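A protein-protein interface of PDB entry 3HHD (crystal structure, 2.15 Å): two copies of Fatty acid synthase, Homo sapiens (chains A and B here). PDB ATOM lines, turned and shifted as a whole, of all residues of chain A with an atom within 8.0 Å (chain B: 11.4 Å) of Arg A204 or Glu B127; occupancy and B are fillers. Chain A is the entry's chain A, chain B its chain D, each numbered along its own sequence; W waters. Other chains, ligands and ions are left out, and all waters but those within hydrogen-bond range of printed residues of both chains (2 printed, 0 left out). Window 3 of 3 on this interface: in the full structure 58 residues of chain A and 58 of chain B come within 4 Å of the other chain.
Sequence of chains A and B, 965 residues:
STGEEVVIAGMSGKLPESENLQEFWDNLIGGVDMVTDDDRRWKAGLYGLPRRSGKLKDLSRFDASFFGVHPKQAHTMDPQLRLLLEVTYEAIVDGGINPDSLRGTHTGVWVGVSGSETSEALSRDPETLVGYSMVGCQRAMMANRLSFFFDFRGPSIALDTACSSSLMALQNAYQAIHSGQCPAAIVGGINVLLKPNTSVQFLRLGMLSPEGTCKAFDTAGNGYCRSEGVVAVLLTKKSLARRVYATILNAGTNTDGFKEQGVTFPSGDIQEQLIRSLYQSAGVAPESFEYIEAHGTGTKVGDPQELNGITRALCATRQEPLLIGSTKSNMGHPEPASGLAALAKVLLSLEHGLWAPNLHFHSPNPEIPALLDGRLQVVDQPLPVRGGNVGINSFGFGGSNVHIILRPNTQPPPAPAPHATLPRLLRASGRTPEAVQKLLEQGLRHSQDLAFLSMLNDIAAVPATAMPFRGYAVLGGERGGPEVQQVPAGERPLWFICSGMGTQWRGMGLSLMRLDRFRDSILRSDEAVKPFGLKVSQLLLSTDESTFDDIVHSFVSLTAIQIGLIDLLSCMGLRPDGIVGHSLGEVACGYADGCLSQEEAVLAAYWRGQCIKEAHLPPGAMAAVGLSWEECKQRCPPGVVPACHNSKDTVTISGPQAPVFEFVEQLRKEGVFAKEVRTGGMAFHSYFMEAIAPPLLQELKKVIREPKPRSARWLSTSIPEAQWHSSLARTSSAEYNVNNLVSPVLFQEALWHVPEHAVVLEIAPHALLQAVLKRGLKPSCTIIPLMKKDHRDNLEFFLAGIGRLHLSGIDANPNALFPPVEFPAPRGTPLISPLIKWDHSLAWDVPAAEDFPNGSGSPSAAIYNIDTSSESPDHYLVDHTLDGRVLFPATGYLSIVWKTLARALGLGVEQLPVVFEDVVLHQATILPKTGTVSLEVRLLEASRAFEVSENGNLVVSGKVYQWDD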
ATOM      1  N   TYR A  47     -15.271   7.838  14.013  1.00  0.00           N
ATOM      2  CA  TYR A  47     -15.538   7.592  15.427  1.00  0.00           C
ATOM      3  C   TYR A  47     -14.736   8.483  16.380  1.00  0.00           C
ATOM      4  O   TYR A  47     -14.554   8.143  17.545  1.00  0.00           O
ATOM      5  CB  TYR A  47     -15.259   6.127  15.743  1.00  0.00           C
ATOM      6  CG  TYR A  47     -15.965   5.162  14.829  1.00  0.00           C
ATOM      7  CD1 TYR A  47     -17.303   5.355  14.462  1.00  0.00           C
ATOM      8  CD2 TYR A  47     -15.336   4.023  14.394  1.00  0.00           C
ATOM      9  CE1 TYR A  47     -17.972   4.448  13.640  1.00  0.00           C
ATOM     10  CE2 TYR A  47     -15.994   3.100  13.571  1.00  0.00           C
ATOM     11  CZ  TYR A  47     -17.312   3.320  13.210  1.00  0.00           C
ATOM     12  OH  TYR A  47     -17.958   2.409  12.423  1.00  0.00           O
ATOM     13  N   GLY A  48     -14.217   9.598  15.884  1.00  0.00           N
ATOM     14  CA  GLY A  48     -13.414  10.475  16.738  1.00  0.00           C
ATOM     15  C   GLY A  48     -11.977   9.995  16.920  1.00  0.00           C
ATOM     16  O   GLY A  48     -11.239  10.452  17.807  1.00  0.00           O
ATOM     17  N   LEU A  49     -11.543   9.105  16.029  1.00  0.00           N
ATOM     18  CA  LEU A  49     -10.191   8.566  16.136  1.00  0.00           C
ATOM     19  C   LEU A  49      -9.167   9.602  15.760  1.00  0.00           C
ATOM     20  O   LEU A  49      -9.469  10.539  15.015  1.00  0.00           O
ATOM     21  CB  LEU A  49     -10.041   7.333  15.226  1.00  0.00           C
ATOM     22  CG  LEU A  49     -10.802   6.113  15.734  1.00  0.00           C
ATOM     23  CD1 LEU A  49     -10.830   5.056  14.661  1.00  0.00           C
ATOM     24  CD2 LEU A  49     -10.167   5.596  17.025  1.00  0.00           C
ATOM     25  N   ASN A 197     -12.563  -0.326  14.786  1.00  0.00           N
ATOM     26  CA  ASN A 197     -13.045  -0.645  16.134  1.00  0.00           C
ATOM     27  C   ASN A 197     -11.883  -0.864  17.101  1.00  0.00           C
ATOM     28  O   ASN A 197     -11.958  -0.446  18.259  1.00  0.00           O
ATOM     29  CB  ASN A 197     -13.929  -1.900  16.114  1.00  0.00           C
ATOM     30  CG  ASN A 197     -14.959  -1.895  14.947  1.00  0.00           C
ATOM     31  OD1 ASN A 197     -14.641  -1.509  13.808  1.00  0.00           O
ATOM     32  ND2 ASN A 197     -16.169  -2.385  15.221  1.00  0.00           N
ATOM     33  N   THR A 198     -10.806  -1.509  16.629  1.00  0.00           N
ATOM     34  CA  THR A 198      -9.643  -1.773  17.483  1.00  0.00           C
ATOM     35  C   THR A 198      -9.034  -0.467  17.984  1.00  0.00           C
ATOM     36  O   THR A 198      -8.658  -0.333  19.147  1.00  0.00           O
ATOM     37  CB  THR A 198      -8.598  -2.631  16.761  1.00  0.00           C
ATOM     38  OG1 THR A 198      -9.222  -3.855  16.337  1.00  0.00           O
ATOM     39  CG2 THR A 198      -7.436  -2.967  17.736  1.00  0.00           C
ATOM     40  N   SER A 199      -8.948   0.513  17.111  1.00  0.00           N
ATOM     41  CA  SER A 199      -8.378   1.796  17.505  1.00  0.00           C
ATOM     42  C   SER A 199      -9.283   2.502  18.503  1.00  0.00           C
ATOM     43  O   SER A 199      -8.800   3.215  19.393  1.00  0.00           O
ATOM     44  CB  SER A 199      -8.158   2.695  16.290  1.00  0.00           C
ATOM     45  OG  SER A 199      -7.076   2.227  15.538  1.00  0.00           O
ATOM     46  N   VAL A 200     -10.597   2.276  18.375  1.00  0.00           N
ATOM     47  CA  VAL A 200     -11.554   2.865  19.305  1.00  0.00           C
ATOM     48  C   VAL A 200     -11.283   2.285  20.698  1.00  0.00           C
ATOM     49  O   VAL A 200     -11.216   3.013  21.699  1.00  0.00           O
ATOM     50  CB  VAL A 200     -13.013   2.678  18.840  1.00  0.00           C
ATOM     51  CG1 VAL A 200     -14.010   3.232  19.866  1.00  0.00           C
ATOM     52  CG2 VAL A 200     -13.230   3.345  17.513  1.00  0.00           C
ATOM     53  N   GLN A 201     -11.044   0.982  20.751  1.00  0.00           N
ATOM     54  CA  GLN A 201     -10.762   0.347  22.035  1.00  0.00           C
ATOM     55  C   GLN A 201      -9.571   1.001  22.718  1.00  0.00           C
ATOM     56  O   GLN A 201      -9.616   1.322  23.908  1.00  0.00           O
ATOM     57  CB  GLN A 201     -10.490  -1.141  21.840  1.00  0.00           C
ATOM     58  CG  GLN A 201     -11.725  -2.013  21.817  1.00  0.00           C
ATOM     59  CD  GLN A 201     -11.382  -3.456  21.510  1.00  0.00           C
ATOM     60  OE1 GLN A 201     -11.672  -4.336  22.307  1.00  0.00           O
ATOM     61  NE2 GLN A 201     -10.746  -3.706  20.352  1.00  0.00           N
ATOM     62  N   PHE A 202      -8.492   1.195  21.967  1.00  0.00           N
ATOM     63  CA  PHE A 202      -7.301   1.814  22.544  1.00  0.00           C
ATOM     64  C   PHE A 202      -7.560   3.266  22.922  1.00  0.00           C
ATOM     65  O   PHE A 202      -7.046   3.767  23.908  1.00  0.00           O
ATOM     66  CB  PHE A 202      -6.107   1.729  21.569  1.00  0.00           C
ATOM     67  CG  PHE A 202      -5.467   0.380  21.522  1.00  0.00           C
ATOM     68  CD1 PHE A 202      -4.891  -0.178  22.668  1.00  0.00           C
ATOM     69  CD2 PHE A 202      -5.448  -0.354  20.337  1.00  0.00           C
ATOM     70  CE1 PHE A 202      -4.257  -1.435  22.619  1.00  0.00           C
ATOM     71  CE2 PHE A 202      -4.815  -1.618  20.273  1.00  0.00           C
ATOM     72  CZ  PHE A 202      -4.213  -2.155  21.397  1.00  0.00           C
ATOM     73  N   LEU A 203      -8.338   3.945  22.108  1.00  0.00           N
ATOM     74  CA  LEU A 203      -8.692   5.347  22.370  1.00  0.00           C
ATOM     75  C   LEU A 203      -9.365   5.449  23.735  1.00  0.00           C
ATOM     76  O   LEU A 203      -8.975   6.241  24.573  1.00  0.00           O
ATOM     77  CB  LEU A 203      -9.649   5.846  21.282  1.00  0.00           C
ATOM     78  CG  LEU A 203     -10.161   7.291  21.416  1.00  0.00           C
ATOM     79  CD1 LEU A 203      -9.016   8.264  21.310  1.00  0.00           C
ATOM     80  CD2 LEU A 203     -11.234   7.581  20.387  1.00  0.00           C
ATOM     81  N   ARG A 204     -10.372   4.620  23.952  1.00  0.00           N
ATOM     82  CA  ARG A 204     -11.101   4.610  25.196  1.00  0.00           C
ATOM     83  C   ARG A 204     -10.299   4.108  26.401  1.00  0.00           C
ATOM     84  O   ARG A 204     -10.597   4.450  27.526  1.00  0.00           O
ATOM     85  CB  ARG A 204     -12.411   3.852  25.024  1.00  0.00           C
ATOM     86  CG  ARG A 204     -13.551   4.833  24.689  1.00  0.00           C
ATOM     87  CD  ARG A 204     -14.683   4.162  24.020  1.00  0.00           C
ATOM     88  NE  ARG A 204     -15.265   5.019  22.991  1.00  0.00           N
ATOM     89  CZ  ARG A 204     -16.299   4.664  22.237  1.00  0.00           C
ATOM     90  NH1 ARG A 204     -16.864   3.473  22.429  1.00  0.00           N
ATOM     91  NH2 ARG A 204     -16.733   5.474  21.272  1.00  0.00           N
ATOM     92  N   LEU A 205      -9.223   3.378  26.170  1.00  0.00           N
ATOM     93  CA  LEU A 205      -8.353   2.967  27.285  1.00  0.00           C
ATOM     94  C   LEU A 205      -7.453   4.136  27.667  1.00  0.00           C
ATOM     95  O   LEU A 205      -6.802   4.083  28.669  1.00  0.00           O
ATOM     96  CB  LEU A 205      -7.451   1.798  26.871  1.00  0.00           C
ATOM     97  CG  LEU A 205      -7.901   0.366  27.160  1.00  0.00           C
ATOM     98  CD1 LEU A 205      -6.927  -0.666  26.600  1.00  0.00           C
ATOM     99  CD2 LEU A 205      -8.107   0.153  28.652  1.00  0.00           C
ATOM    100  N   GLY A 206      -7.403   5.175  26.841  1.00  0.00           N
ATOM    101  CA  GLY A 206      -6.521   6.318  27.070  1.00  0.00           C
ATOM    102  C   GLY A 206      -5.082   6.106  26.590  1.00  0.00           C
ATOM    103  O   GLY A 206      -4.130   6.784  27.016  1.00  0.00           O
ATOM    104  N   MET A 207      -4.897   5.147  25.688  1.00  0.00           N
ATOM    105  CA  MET A 207      -3.549   4.836  25.213  1.00  0.00           C
ATOM    106  C   MET A 207      -3.102   5.586  23.969  1.00  0.00           C
ATOM    107  O   MET A 207      -1.913   5.639  23.693  1.00  0.00           O
ATOM    108  CB  MET A 207      -3.404   3.329  24.996  1.00  0.00           C
ATOM    109  CG  MET A 207      -3.450   2.548  26.298  1.00  0.00           C
ATOM    110  SD  MET A 207      -3.504   0.837  25.970  1.00  0.00           S
ATOM    111  CE  MET A 207      -3.299   0.106  27.718  1.00  0.00           C
ATOM    112  N   LEU A 208      -4.051   6.148  23.213  1.00  0.00           N
ATOM    113  CA  LEU A 208      -3.714   6.868  21.983  1.00  0.00           C
ATOM    114  C   LEU A 208      -3.550   8.373  22.141  1.00  0.00           C
ATOM    115  O   LEU A 208      -4.389   9.048  22.720  1.00  0.00           O
ATOM    116  CB  LEU A 208      -4.777   6.630  20.909  1.00  0.00           C
ATOM    117  CG  LEU A 208      -5.042   5.183  20.532  1.00  0.00           C
ATOM    118  CD1 LEU A 208      -5.919   5.155  19.278  1.00  0.00           C
ATOM    119  CD2 LEU A 208      -3.705   4.435  20.318  1.00  0.00           C
ATOM    120  N   ASN A 854     -20.300  -2.267  12.593  1.00  0.00           N
ATOM    121  CA  ASN A 854     -20.269  -0.860  12.984  1.00  0.00           C
ATOM    122  C   ASN A 854     -21.405  -0.477  13.939  1.00  0.00           C
ATOM    123  O   ASN A 854     -22.131  -1.332  14.463  1.00  0.00           O
ATOM    124  CB  ASN A 854     -20.269   0.055  11.759  1.00  0.00           C
ATOM    125  CG  ASN A 854     -21.516  -0.118  10.899  1.00  0.00           C
ATOM    126  OD1 ASN A 854     -21.644   0.511   9.854  1.00  0.00           O
ATOM    127  ND2 ASN A 854     -22.443  -0.961  11.346  1.00  0.00           N
ATOM    128  N   GLN B  73     -15.650  -4.916  34.785  1.00  0.00           N
ATOM    129  CA  GLN B  73     -14.593  -5.641  34.074  1.00  0.00           C
ATOM    130  C   GLN B  73     -14.911  -7.147  33.959  1.00  0.00           C
ATOM    131  O   GLN B  73     -14.656  -7.784  32.930  1.00  0.00           O
ATOM    132  CB  GLN B  73     -13.233  -5.418  34.748  1.00  0.00           C
ATOM    133  CG  GLN B  73     -12.662  -4.018  34.510  1.00  0.00           C
ATOM    134  CD  GLN B  73     -13.453  -2.894  35.214  1.00  0.00           C
ATOM    135  OE1 GLN B  73     -13.824  -3.007  36.379  1.00  0.00           O
ATOM    136  NE2 GLN B  73     -13.696  -1.803  34.497  1.00  0.00           N
ATOM    137  N   THR B  76     -16.959  -8.032  31.001  1.00  0.00           N
ATOM    138  CA  THR B  76     -16.252  -7.817  29.720  1.00  0.00           C
ATOM    139  C   THR B  76     -14.927  -8.589  29.627  1.00  0.00           C
ATOM    140  O   THR B  76     -14.038  -8.204  28.900  1.00  0.00           O
ATOM    141  CB  THR B  76     -16.020  -6.308  29.461  1.00  0.00           C
ATOM    142  OG1 THR B  76     -15.347  -5.751  30.594  1.00  0.00           O
ATOM    143  CG2 THR B  76     -17.390  -5.566  29.272  1.00  0.00           C
ATOM    144  N   ALA B 121     -16.839 -10.078  19.643  1.00  0.00           N
ATOM    145  CA  ALA B 121     -18.205  -9.724  20.065  1.00  0.00           C
ATOM    146  C   ALA B 121     -18.231  -8.382  20.802  1.00  0.00           C
ATOM    147  O   ALA B 121     -19.118  -7.550  20.586  1.00  0.00           O
ATOM    148  CB  ALA B 121     -18.760 -10.811  20.995  1.00  0.00           C
ATOM    149  N   LEU B 122     -17.238  -8.167  21.661  1.00  0.00           N
ATOM    150  CA  LEU B 122     -17.192  -6.966  22.483  1.00  0.00           C
ATOM    151  C   LEU B 122     -16.686  -5.703  21.809  1.00  0.00           C
ATOM    152  O   LEU B 122     -16.797  -4.616  22.363  1.00  0.00           O
ATOM    153  CB  LEU B 122     -16.402  -7.236  23.775  1.00  0.00           C
ATOM    154  CG  LEU B 122     -17.026  -8.240  24.737  1.00  0.00           C
ATOM    155  CD1 LEU B 122     -16.179  -8.308  26.026  1.00  0.00           C
ATOM    156  CD2 LEU B 122     -18.457  -7.842  25.039  1.00  0.00           C
ATOM    157  N   SER B 123     -16.092  -5.825  20.634  1.00  0.00           N
ATOM    158  CA  SER B 123     -15.615  -4.623  19.948  1.00  0.00           C
ATOM    159  C   SER B 123     -16.519  -4.334  18.740  1.00  0.00           C
ATOM    160  O   SER B 123     -16.154  -3.532  17.862  1.00  0.00           O
ATOM    161  CB  SER B 123     -14.174  -4.813  19.466  1.00  0.00           C
ATOM    162  OG  SER B 123     -14.089  -5.954  18.625  1.00  0.00           O
ATOM    163  N   ARG B 124     -17.652  -5.041  18.654  1.00  0.00           N
ATOM    164  CA  ARG B 124     -18.554  -4.885  17.489  1.00  0.00           C
ATOM    165  C   ARG B 124     -19.254  -3.533  17.348  1.00  0.00           C
ATOM    166  O   ARG B 124     -19.633  -3.142  16.247  1.00  0.00           O
ATOM    167  CB  ARG B 124     -19.577  -6.024  17.393  1.00  0.00           C
ATOM    168  CG  ARG B 124     -20.748  -5.901  18.389  1.00  0.00           C
ATOM    169  CD  ARG B 124     -21.535  -7.207  18.399  1.00  0.00           C
ATOM    170  NE  ARG B 124     -22.757  -7.165  19.234  1.00  0.00           N
ATOM    171  CZ  ARG B 124     -22.775  -7.404  20.555  1.00  0.00           C
ATOM    172  NH1 ARG B 124     -21.650  -7.692  21.219  1.00  0.00           N
ATOM    173  NH2 ARG B 124     -23.916  -7.376  21.230  1.00  0.00           N
ATOM    174  N   ASP B 125     -19.461  -2.836  18.463  1.00  0.00           N
ATOM    175  CA  ASP B 125     -20.190  -1.561  18.459  1.00  0.00           C
ATOM    176  C   ASP B 125     -19.311  -0.407  18.892  1.00  0.00           C
ATOM    177  O   ASP B 125     -19.096  -0.195  20.075  1.00  0.00           O
ATOM    178  CB  ASP B 125     -21.379  -1.663  19.416  1.00  0.00           C
ATOM    179  CG  ASP B 125     -22.431  -0.576  19.175  1.00  0.00           C
ATOM    180  OD1 ASP B 125     -22.064   0.547  18.761  1.00  0.00           O
ATOM    181  OD2 ASP B 125     -23.630  -0.864  19.401  1.00  0.00           O
ATOM    182  N   PRO B 126     -18.808   0.372  17.935  1.00  0.00           N
ATOM    183  CA  PRO B 126     -17.854   1.454  18.217  1.00  0.00           C
ATOM    184  C   PRO B 126     -18.416   2.534  19.122  1.00  0.00           C
ATOM    185  O   PRO B 126     -17.683   3.177  19.888  1.00  0.00           O
ATOM    186  CB  PRO B 126     -17.512   2.020  16.819  1.00  0.00           C
ATOM    187  CG  PRO B 126     -18.423   1.317  15.837  1.00  0.00           C
ATOM    188  CD  PRO B 126     -18.934   0.078  16.494  1.00  0.00           C
ATOM    189  N   GLU B 127     -19.722   2.744  19.022  1.00  0.00           N
ATOM    190  CA  GLU B 127     -20.373   3.759  19.822  1.00  0.00           C
ATOM    191  C   GLU B 127     -20.459   3.364  21.283  1.00  0.00           C
ATOM    192  O   GLU B 127     -20.270   4.199  22.160  1.00  0.00           O
ATOM    193  CB  GLU B 127     -21.769   4.048  19.273  1.00  0.00           C
ATOM    194  CG  GLU B 127     -21.721   4.960  18.039  1.00  0.00           C
ATOM    195  CD  GLU B 127     -22.320   6.323  18.303  1.00  0.00           C
ATOM    196  OE1 GLU B 127     -23.560   6.431  18.267  1.00  0.00           O
ATOM    197  OE2 GLU B 127     -21.549   7.245  18.644  1.00  0.00           O
ATOM    198  N   THR B 128     -20.702   2.085  21.546  1.00  0.00           N
ATOM    199  CA  THR B 128     -20.828   1.621  22.924  1.00  0.00           C
ATOM    200  C   THR B 128     -19.653   0.830  23.537  1.00  0.00           C
ATOM    201  O   THR B 128     -19.618   0.625  24.759  1.00  0.00           O
ATOM    202  CB  THR B 128     -22.122   0.862  23.140  1.00  0.00           C
ATOM    203  OG1 THR B 128     -22.035  -0.422  22.518  1.00  0.00           O
ATOM    204  CG2 THR B 128     -23.297   1.634  22.562  1.00  0.00           C
ATOM    205  N   LEU B 129     -18.714   0.355  22.724  1.00  0.00           N
ATOM    206  CA  LEU B 129     -17.656  -0.498  23.270  1.00  0.00           C
ATOM    207  C   LEU B 129     -16.864   0.245  24.326  1.00  0.00           C
ATOM    208  O   LEU B 129     -16.766   1.466  24.301  1.00  0.00           O
ATOM    209  CB  LEU B 129     -16.764  -1.092  22.172  1.00  0.00           C
ATOM    210  CG  LEU B 129     -15.847  -0.142  21.417  1.00  0.00           C
ATOM    211  CD1 LEU B 129     -14.617   0.161  22.242  1.00  0.00           C
ATOM    212  CD2 LEU B 129     -15.494  -0.752  20.039  1.00  0.00           C
ATOM    213  N   VAL B 130     -16.346  -0.495  25.293  1.00  0.00           N
ATOM    214  CA  VAL B 130     -15.539   0.107  26.328  1.00  0.00           C
ATOM    215  C   VAL B 130     -14.100  -0.362  26.154  1.00  0.00           C
ATOM    216  O   VAL B 130     -13.841  -1.479  25.684  1.00  0.00           O
ATOM    217  CB  VAL B 130     -16.098  -0.271  27.745  1.00  0.00           C
ATOM    218  CG1 VAL B 130     -17.486   0.367  27.984  1.00  0.00           C
ATOM    219  CG2 VAL B 130     -16.131  -1.800  27.914  1.00  0.00           C
ATOM    220  N   GLY B 131     -13.174   0.451  26.634  1.00  0.00           N
ATOM    221  CA  GLY B 131     -11.759   0.169  26.548  1.00  0.00           C
ATOM    222  C   GLY B 131     -11.317  -1.052  27.345  1.00  0.00           C
ATOM    223  O   GLY B 131     -10.466  -1.833  26.870  1.00  0.00           O
ATOM    224  N   TYR B 132     -11.896  -1.257  28.527  1.00  0.00           N
ATOM    225  CA  TYR B 132     -11.471  -2.403  29.346  1.00  0.00           C
ATOM    226  C   TYR B 132     -11.797  -3.784  28.785  1.00  0.00           C
ATOM    227  O   TYR B 132     -11.337  -4.801  29.312  1.00  0.00           O
ATOM    228  CB  TYR B 132     -11.855  -2.274  30.827  1.00  0.00           C
ATOM    229  CG  TYR B 132     -13.244  -1.739  31.068  1.00  0.00           C
ATOM    230  CD1 TYR B 132     -13.456  -0.364  31.295  1.00  0.00           C
ATOM    231  CD2 TYR B 132     -14.349  -2.599  31.078  1.00  0.00           C
ATOM    232  CE1 TYR B 132     -14.736   0.130  31.527  1.00  0.00           C
ATOM    233  CE2 TYR B 132     -15.641  -2.103  31.280  1.00  0.00           C
ATOM    234  CZ  TYR B 132     -15.824  -0.753  31.522  1.00  0.00           C
ATOM    235  OH  TYR B 132     -17.092  -0.285  31.754  1.00  0.00           O
ATOM    236  N   SER B 133     -12.532  -3.840  27.683  1.00  0.00           N
ATOM    237  CA  SER B 133     -12.769  -5.145  27.085  1.00  0.00           C
ATOM    238  C   SER B 133     -11.449  -5.670  26.465  1.00  0.00           C
ATOM    239  O   SER B 133     -11.251  -6.882  26.312  1.00  0.00           O
ATOM    240  CB  SER B 133     -13.912  -5.105  26.061  1.00  0.00           C
ATOM    241  OG  SER B 133     -13.607  -4.224  24.976  1.00  0.00           O
ATOM    242  N   MET B 134     -10.531  -4.754  26.153  1.00  0.00           N
ATOM    243  CA  MET B 134      -9.222  -5.117  25.591  1.00  0.00           C
ATOM    244  C   MET B 134      -8.380  -5.789  26.678  1.00  0.00           C
ATOM    245  O   MET B 134      -7.750  -6.810  26.454  1.00  0.00           O
ATOM    246  CB  MET B 134      -8.537  -3.878  25.041  1.00  0.00           C
ATOM    247  CG  MET B 134      -7.113  -4.072  24.625  1.00  0.00           C
ATOM    248  SD  MET B 134      -6.972  -4.786  22.947  1.00  0.00           S
ATOM    249  CE  MET B 134      -6.943  -3.237  21.992  1.00  0.00           C
ATOM    250  N   VAL B 135      -8.455  -5.251  27.885  1.00  0.00           N
ATOM    251  CA  VAL B 135      -7.762  -5.803  29.046  1.00  0.00           C
ATOM    252  C   VAL B 135      -8.285  -7.203  29.478  1.00  0.00           C
ATOM    253  O   VAL B 135      -7.549  -8.022  30.038  1.00  0.00           O
ATOM    254  CB  VAL B 135      -7.815  -4.788  30.227  1.00  0.00           C
ATOM    255  CG1 VAL B 135      -7.171  -5.368  31.484  1.00  0.00           C
ATOM    256  CG2 VAL B 135      -7.160  -3.449  29.801  1.00  0.00           C
HETATM  257  O   HOH W   1     -17.912   3.681  25.633  1.00  0.00           O
HETATM  258  O   HOH W   2     -12.390   2.077  29.067  1.00  0.00           O
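ND2 of Asn A197 sits at hydrogen-bond distance from O of Ser B123 (2.9 Å). The side-chain amide oxygen (OE1) of Gln A201 is in hydrogen-bond range of the side-chain hydroxyl (OG) of Ser B133 (3.3 Å). The guanidinium group (NH1) of Arg A204 sits at hydrogen-bond distance from the backbone carbonyl oxygen (O) of Pro B126, at 2.7 Å. O of Glu B127 sits at hydrogen-bond distance from NH1 of Arg A204 (3.5 Å). NH1 of Arg A204 is in hydrogen-bond range of O of Leu B129, at 2.7 Å.
O of Phe A202 is in hydrogen-bond range of N of Met A207, 3.1 Å away. The backbone carbonyl oxygen of Ala B121 is in hydrogen-bond range of the guanidinium group of Arg B124, 2.6 Å away. N of Glu B127 sits close to OD1 of Asp B125, 3.2 Å away. OD1 of Asp B125 is in hydrogen-bond range of N of Thr B128, 3.5 Å away. O of Val B130 lies within hydrogen-bond range of OG of Ser B133.
Among the printed residues, merely in contact across the chains: Phe A202 with Met B134 (3.0 Å), Leu A205 with Gly B131 (3.4 Å), Tyr A47 with Pro B126 (3.5 Å), Asn A854 with Arg B124 (3.6 Å), Gln A201 with Gly B131 (3.6 Å), Asn A854 with Pro B126 (3.6 Å), Gln A201 with Leu B129 (3.6 Å), Val A200 with Pro B126 (3.7 Å), Asn A197 with Arg B124 (3.7 Å), Gln A201 with Ser B123 (3.7 Å), Arg A204 with Gly B131 (3.8 Å), Leu A205 with Val B135 (3.9 Å), Asn A197 with Pro B126 (3.9 Å), Leu A205 with Met B134 (3.9 Å), Val A200 with Leu B129 (3.9 Å), Asn A197 with Leu B129 (3.97 Å) and Arg A204 with Thr B128 (3.999 Å).
Printed residues of chain B within 4 Å of Arg A204: Pro B126 (2.7 Å), Glu B127 (3.5 Å), Thr B128 (3.999 Å), Leu B129 (2.7 Å) and Gly B131 (3.8 Å). Glu B127 touches one residue of chain A. Val A200 touches just these residues of chain B: Pro B126 and Leu B129. No residue of chain B comes within 4 Å of Leu A203. Leu A205 touches three residues of chain B. No residue of chain B comes within 4 Å of Gly A206. Of the printed residues of chain A, Pro B126 touches Tyr A47 (3.5 Å), Asn A197 (3.9 Å), Val A200 (3.7 Å), Arg A204 (2.7 Å) and Asn A854 (3.6 Å). Of the printed residues of chain A, Leu B129 touches Asn A197 (3.97 Å), Val A200 (3.9 Å), Gln A201 (3.6 Å) and Arg A204 (2.7 Å). Of the printed residues of chain A, Met B134 touches Phe A202 and Leu A205. Of the printed residues of chain A, Arg B124 touches Asn A197 (3.7 Å) and Asn A854 (3.6 Å). Of the printed residues of chain A, Ser B133 touches Gln A201 (3.3 Å). Ala B121 touches none of the printed residues of chain A.
Of the 16 printed residues of chain A, 8 touch a printed residue of chain B. Printed residues of chain A that touch a printed residue of chain B: Tyr A47, Asn A197, Val A200, Gln A201, Phe A202, Arg A204, Leu A205 and Asn A854. Hydrophobic or aromatic side chains of chain A that line the printed part of chain B: Tyr A47, Val A200, Phe A202 and Leu A205. Of the 17 printed residues of chain B, 10 touch a printed residue of chain A. Among the printed residues, no Asp or Glu carboxylate lies within 4 Å of a Lys or Arg side-chain nitrogen of the other chain.
No position is printed for both chains. Of the 22 pairs that touch across the chains among the printed residues, none has its exchanged pair printed and touching as well.
Water W1 bridges O of Leu B129 (2.8 Å) and NH1 of Arg A204 (3.4 Å). Water W2 lies within hydrogen-bond range of the backbone NH (N) of Gly B131 (3.0 Å), the backbone carbonyl oxygen (O) of Arg A204 (3.3 Å) and the backbone NH (N) of Tyr B132 (3.4 Å).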
